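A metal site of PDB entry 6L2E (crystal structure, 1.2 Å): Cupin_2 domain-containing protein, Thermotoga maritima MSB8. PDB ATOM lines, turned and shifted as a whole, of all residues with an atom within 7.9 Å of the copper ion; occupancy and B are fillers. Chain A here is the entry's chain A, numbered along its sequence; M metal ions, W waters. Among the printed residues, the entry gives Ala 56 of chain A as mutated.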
ATOM      1  N   ARG A  43      -2.907  -4.725   6.964  1.00  0.00           N
ATOM      2  CA  ARG A  43      -3.119  -5.402   5.691  1.00  0.00           C
ATOM      3  C   ARG A  43      -2.899  -6.899   5.863  1.00  0.00           C
ATOM      4  O   ARG A  43      -2.132  -7.308   6.730  1.00  0.00           O
ATOM      5  CB  ARG A  43      -2.166  -4.880   4.618  1.00  0.00           C
ATOM      6  CG  ARG A  43      -2.274  -3.391   4.331  1.00  0.00           C
ATOM      7  CD  ARG A  43      -1.361  -2.525   5.136  1.00  0.00           C
ATOM      8  NE  ARG A  43       0.056  -2.871   5.100  1.00  0.00           N
ATOM      9  CZ  ARG A  43       0.943  -2.581   4.171  1.00  0.00           C
ATOM     10  NH1 ARG A  43       2.211  -2.971   4.280  1.00  0.00           N
ATOM     11  NH2 ARG A  43       0.617  -1.879   3.091  1.00  0.00           N
ATOM     12  N   ILE A  53       8.320 -10.567  -3.141  1.00  0.00           N
ATOM     13  CA  ILE A  53       8.423  -9.195  -2.703  1.00  0.00           C
ATOM     14  C   ILE A  53       9.916  -8.923  -2.542  1.00  0.00           C
ATOM     15  O   ILE A  53      10.520  -9.292  -1.547  1.00  0.00           O
ATOM     16  CB  ILE A  53       7.659  -8.986  -1.389  1.00  0.00           C
ATOM     17  CG1 ILE A  53       6.174  -9.335  -1.545  1.00  0.00           C
ATOM     18  CG2 ILE A  53       7.814  -7.574  -0.855  1.00  0.00           C
ATOM     19  CD1 ILE A  53       5.416  -9.421  -0.243  1.00  0.00           C
ATOM     20  N   ASP A  54      10.506  -8.349  -3.590  1.00  0.00           N
ATOM     21  CA  ASP A  54      11.974  -8.361  -3.639  1.00  0.00           C
ATOM     22  C   ASP A  54      12.542  -7.353  -2.661  1.00  0.00           C
ATOM     23  O   ASP A  54      11.856  -6.450  -2.153  1.00  0.00           O
ATOM     24  CB  ASP A  54      12.446  -8.153  -5.068  1.00  0.00           C
ATOM     25  CG  ASP A  54      13.775  -8.820  -5.361  1.00  0.00           C
ATOM     26  OD1 ASP A  54      14.413  -9.404  -4.465  1.00  0.00           O
ATOM     27  OD2 ASP A  54      14.199  -8.761  -6.538  1.00  0.00           O
ATOM     28  N   ARG A  55      13.827  -7.549  -2.365  1.00  0.00           N
ATOM     29  CA  ARG A  55      14.514  -6.728  -1.377  1.00  0.00           C
ATOM     30  C   ARG A  55      14.338  -5.237  -1.637  1.00  0.00           C
ATOM     31  O   ARG A  55      14.518  -4.742  -2.757  1.00  0.00           O
ATOM     32  CB  ARG A  55      16.005  -7.057  -1.372  1.00  0.00           C
ATOM     33  CG  ARG A  55      16.348  -8.358  -0.643  1.00  0.00           C
ATOM     34  CD  ARG A  55      17.837  -8.583  -0.639  1.00  0.00           C
ATOM     35  NE  ARG A  55      18.220  -9.794   0.074  1.00  0.00           N
ATOM     36  CZ  ARG A  55      18.239 -11.021  -0.407  1.00  0.00           C
ATOM     37  NH1 ARG A  55      17.891 -11.314  -1.660  1.00  0.00           N
ATOM     38  NH2 ARG A  55      18.638 -11.980   0.441  1.00  0.00           N
ATOM     39  N   ALA A  56      14.020  -4.528  -0.576  1.00  0.00           N
ATOM     40  CA  ALA A  56      13.828  -3.100  -0.600  1.00  0.00           C
ATOM     41  C   ALA A  56      14.044  -2.555   0.812  1.00  0.00           C
ATOM     42  O   ALA A  56      14.161  -3.306   1.801  1.00  0.00           O
ATOM     43  CB  ALA A  56      12.438  -2.726  -1.098  1.00  0.00           C
ATOM     44  N   SER A  57      14.058  -1.237   0.869  1.00  0.00           N
ATOM     45  CA  SER A  57      14.036  -0.571   2.175  1.00  0.00           C
ATOM     46  C   SER A  57      13.241   0.725   2.030  1.00  0.00           C
ATOM     47  O   SER A  57      13.078   1.260   0.938  1.00  0.00           O
ATOM     48  CB  SER A  57      15.449  -0.316   2.683  1.00  0.00           C
ATOM     49  OG  SER A  57      16.141   0.594   1.869  1.00  0.00           O
ATOM     50  N   HIS A  58      12.732   1.175   3.175  1.00  0.00           N
ATOM     51  CA  HIS A  58      11.872   2.360   3.181  1.00  0.00           C
ATOM     52  C   HIS A  58      11.902   2.948   4.586  1.00  0.00           C
ATOM     53  O   HIS A  58      12.160   2.251   5.550  1.00  0.00           O
ATOM     54  CB  HIS A  58      10.451   2.068   2.741  1.00  0.00           C
ATOM     55  CG  HIS A  58       9.901   0.766   3.220  1.00  0.00           C
ATOM     56  ND1 HIS A  58       9.661   0.481   4.541  1.00  0.00           N
ATOM     57  CD2 HIS A  58       9.556  -0.353   2.538  1.00  0.00           C
ATOM     58  CE1 HIS A  58       9.184  -0.754   4.642  1.00  0.00           C
ATOM     59  NE2 HIS A  58       9.078  -1.304   3.451  1.00  0.00           N
ATOM     60  N   TRP A  60      10.087   3.586   7.048  1.00  0.00           N
ATOM     61  CA  TRP A  60       9.130   3.165   8.050  1.00  0.00           C
ATOM     62  C   TRP A  60       9.337   1.680   8.310  1.00  0.00           C
ATOM     63  O   TRP A  60       9.860   0.961   7.464  1.00  0.00           O
ATOM     64  CB  TRP A  60       7.680   3.452   7.638  1.00  0.00           C
ATOM     65  CG  TRP A  60       7.252   2.791   6.373  1.00  0.00           C
ATOM     66  CD1 TRP A  60       6.749   1.527   6.203  1.00  0.00           C
ATOM     67  CD2 TRP A  60       7.284   3.382   5.065  1.00  0.00           C
ATOM     68  NE1 TRP A  60       6.475   1.296   4.871  1.00  0.00           N
ATOM     69  CE2 TRP A  60       6.797   2.423   4.152  1.00  0.00           C
ATOM     70  CE3 TRP A  60       7.681   4.630   4.590  1.00  0.00           C
ATOM     71  CZ2 TRP A  60       6.690   2.684   2.791  1.00  0.00           C
ATOM     72  CZ3 TRP A  60       7.591   4.901   3.228  1.00  0.00           C
ATOM     73  CH2 TRP A  60       7.095   3.921   2.350  1.00  0.00           C
ATOM     74  N   GLU A  61       8.902   1.274   9.494  1.00  0.00           N
ATOM     75  CA  GLU A  61       8.974  -0.088   9.970  1.00  0.00           C
ATOM     76  C   GLU A  61       7.829  -0.956   9.451  1.00  0.00           C
ATOM     77  O   GLU A  61       6.806  -0.451   9.003  1.00  0.00           O
ATOM     78  CB  GLU A  61       8.913  -0.113  11.512  1.00  0.00           C
ATOM     79  CG  GLU A  61       7.597   0.274  12.157  1.00  0.00           C
ATOM     80  CD  GLU A  61       7.333   1.751  12.335  1.00  0.00           C
ATOM     81  OE1 GLU A  61       8.007   2.592  11.687  1.00  0.00           O
ATOM     82  OE2 GLU A  61       6.405   2.102  13.125  1.00  0.00           O
ATOM     83  N   HIS A  62       8.047  -2.253   9.572  1.00  0.00           N
ATOM     84  CA  HIS A  62       7.020  -3.260   9.443  1.00  0.00           C
ATOM     85  C   HIS A  62       6.857  -4.047  10.744  1.00  0.00           C
ATOM     86  O   HIS A  62       7.834  -4.405  11.395  1.00  0.00           O
ATOM     87  CB  HIS A  62       7.297  -4.324   8.378  1.00  0.00           C
ATOM     88  CG  HIS A  62       7.244  -3.966   6.939  1.00  0.00           C
ATOM     89  ND1 HIS A  62       6.071  -3.623   6.313  1.00  0.00           N
ATOM     90  CD2 HIS A  62       8.193  -3.927   5.991  1.00  0.00           C
ATOM     91  CE1 HIS A  62       6.312  -3.375   5.039  1.00  0.00           C
ATOM     92  NE2 HIS A  62       7.594  -3.550   4.801  1.00  0.00           N
ATOM     93  N   ILE A  64       4.893  -7.665  11.375  1.00  0.00           N
ATOM     94  CA  ILE A  64       4.334  -8.747  10.575  1.00  0.00           C
ATOM     95  C   ILE A  64       4.021  -9.947  11.472  1.00  0.00           C
ATOM     96  O   ILE A  64       4.761 -10.239  12.407  1.00  0.00           O
ATOM     97  CB  ILE A  64       5.293  -9.153   9.451  1.00  0.00           C
ATOM     98  CG1 ILE A  64       5.306  -8.077   8.362  1.00  0.00           C
ATOM     99  CG2 ILE A  64       4.966 -10.514   8.859  1.00  0.00           C
ATOM    100  CD1 ILE A  64       6.475  -8.183   7.401  1.00  0.00           C
ATOM    101  N   VAL A  90      10.667  -5.362  11.303  1.00  0.00           N
ATOM    102  CA  VAL A  90      11.671  -4.806  10.409  1.00  0.00           C
ATOM    103  C   VAL A  90      11.824  -3.333  10.747  1.00  0.00           C
ATOM    104  O   VAL A  90      10.869  -2.562  10.627  1.00  0.00           O
ATOM    105  CB  VAL A  90      11.262  -4.960   8.933  1.00  0.00           C
ATOM    106  CG1 VAL A  90      12.429  -4.573   8.017  1.00  0.00           C
ATOM    107  CG2 VAL A  90      10.815  -6.384   8.583  1.00  0.00           C
ATOM    108  N   GLU A  94      15.760  -0.924   7.059  1.00  0.00           N
ATOM    109  CA  GLU A  94      16.422  -2.234   7.008  1.00  0.00           C
ATOM    110  C   GLU A  94      16.037  -2.935   5.712  1.00  0.00           C
ATOM    111  O   GLU A  94      14.860  -2.954   5.382  1.00  0.00           O
ATOM    112  CB  GLU A  94      15.983  -3.076   8.206  1.00  0.00           C
ATOM    113  CG  GLU A  94      16.698  -4.390   8.372  1.00  0.00           C
ATOM    114  CD  GLU A  94      18.177  -4.302   8.640  1.00  0.00           C
ATOM    115  OE1 GLU A  94      18.903  -5.243   8.223  1.00  0.00           O
ATOM    116  OE2 GLU A  94      18.736  -3.345   9.250  1.00  0.00           O
ATOM    117  N   ILE A  95      17.008  -3.509   5.029  1.00  0.00           N
ATOM    118  CA  ILE A  95      16.710  -4.269   3.820  1.00  0.00           C
ATOM    119  C   ILE A  95      15.900  -5.518   4.155  1.00  0.00           C
ATOM    120  O   ILE A  95      16.174  -6.245   5.105  1.00  0.00           O
ATOM    121  CB  ILE A  95      18.010  -4.639   3.079  1.00  0.00           C
ATOM    122  CG1 ILE A  95      18.679  -3.399   2.485  1.00  0.00           C
ATOM    123  CG2 ILE A  95      17.788  -5.662   1.976  1.00  0.00           C
ATOM    124  CD1 ILE A  95      20.157  -3.537   2.217  1.00  0.00           C
ATOM    125  N   HIS A  96      14.835  -5.768   3.395  1.00  0.00           N
ATOM    126  CA  HIS A  96      13.987  -6.925   3.608  1.00  0.00           C
ATOM    127  C   HIS A  96      13.224  -7.241   2.333  1.00  0.00           C
ATOM    128  O   HIS A  96      12.991  -6.368   1.509  1.00  0.00           O
ATOM    129  CB  HIS A  96      12.970  -6.677   4.751  1.00  0.00           C
ATOM    130  CG  HIS A  96      12.062  -5.534   4.377  1.00  0.00           C
ATOM    131  ND1 HIS A  96      12.476  -4.217   4.379  1.00  0.00           N
ATOM    132  CD2 HIS A  96      10.780  -5.485   3.937  1.00  0.00           C
ATOM    133  CE1 HIS A  96      11.485  -3.440   3.961  1.00  0.00           C
ATOM    134  NE2 HIS A  96      10.432  -4.176   3.685  1.00  0.00           N
ATOM    135  N   GLY A  97      12.795  -8.486   2.214  1.00  0.00           N
ATOM    136  CA  GLY A  97      11.893  -8.934   1.184  1.00  0.00           C
ATOM    137  C   GLY A  97      11.335 -10.292   1.591  1.00  0.00           C
ATOM    138  O   GLY A  97      11.691 -10.806   2.645  1.00  0.00           O
ATOM    139  N   PHE A  98      10.503 -10.861   0.740  1.00  0.00           N
ATOM    140  CA  PHE A  98       9.811 -12.099   1.027  1.00  0.00           C
ATOM    141  C   PHE A  98       9.613 -12.922  -0.247  1.00  0.00           C
ATOM    142  O   PHE A  98       9.472 -12.385  -1.338  1.00  0.00           O
ATOM    143  CB  PHE A  98       8.438 -11.874   1.681  1.00  0.00           C
ATOM    144  CG  PHE A  98       8.546 -10.926   2.855  1.00  0.00           C
ATOM    145  CD1 PHE A  98       8.974 -11.382   4.085  1.00  0.00           C
ATOM    146  CD2 PHE A  98       8.219  -9.585   2.690  1.00  0.00           C
ATOM    147  CE1 PHE A  98       9.075 -10.498   5.149  1.00  0.00           C
ATOM    148  CE2 PHE A  98       8.330  -8.697   3.743  1.00  0.00           C
ATOM    149  CZ  PHE A  98       8.763  -9.162   4.975  1.00  0.00           C
ATOM    150  N   CSD A 110       0.433  -7.529   7.951  1.00  0.00           N
ATOM    151  CA  CSD A 110       1.556  -6.564   7.797  1.00  0.00           C
ATOM    152  CB  CSD A 110       2.023  -6.555   6.335  1.00  0.00           C
ATOM    153  SG  CSD A 110       3.552  -5.619   6.143  1.00  0.00           S
ATOM    154  C   CSD A 110       0.956  -5.183   8.163  1.00  0.00           C
ATOM    155  O   CSD A 110       0.007  -4.722   7.584  1.00  0.00           O
ATOM    156  OD1 CSD A 110       4.077  -5.904   4.588  1.00  0.00           O
ATOM    157  OD2 CSD A 110       3.162  -4.266   6.309  1.00  0.00           O
ATOM    158  N   ILE A 112       2.011  -1.105   9.137  1.00  0.00           N
ATOM    159  CA  ILE A 112       2.953  -0.028   8.954  1.00  0.00           C
ATOM    160  C   ILE A 112       2.331   1.253   9.512  1.00  0.00           C
ATOM    161  O   ILE A 112       1.112   1.392   9.526  1.00  0.00           O
ATOM    162  CB  ILE A 112       3.341   0.180   7.481  1.00  0.00           C
ATOM    163  CG1 ILE A 112       2.135   0.523   6.568  1.00  0.00           C
ATOM    164  CG2 ILE A 112       4.101  -1.020   6.922  1.00  0.00           C
ATOM    165  CD1 ILE A 112       2.528   0.852   5.152  1.00  0.00           C
HETATM  166 CU    CU M   1       8.674  -3.268   3.107  1.00  0.00          CU
HETATM  167  O   HOH W   1       7.879  -4.707   1.960  1.00  0.00           O
HETATM  168  O   HOH W   2       9.491  -3.230   1.276  1.00  0.00           O
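Three residues have an atom within 4 Å of the copper ion: His 58, His 62 and His 96. The nearest printed residue that does not touch the copper ion is Trp 60 (5.4 Å).
The copper ion is bound by water W1. The copper ion is bound by water W2 (2.0 Å). The copper ion is bound by a ring nitrogen (NE2) of His 62 (2.0 Å). The copper ion is bound by NE2 of His 58 (2.0 Å). The copper ion is bound by NE2 of His 96, 2.1 Å away. The copper ion has five donor atoms within binding distance.
ND1 of His 62 lies within hydrogen-bond range of OD2 of CSD 110 (3.0 Å). O of His 62 lies within hydrogen-bond range of N of Val 90 (3.0 Å). ND1 of His 58 is in hydrogen-bond range of O of Trp 60, 3.0 Å away. O of His 96 sits at hydrogen-bond distance from N of Ala 56 (3.0 Å). O of Glu 94 is in hydrogen-bond range of ND1 of His 96 (2.9 Å).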
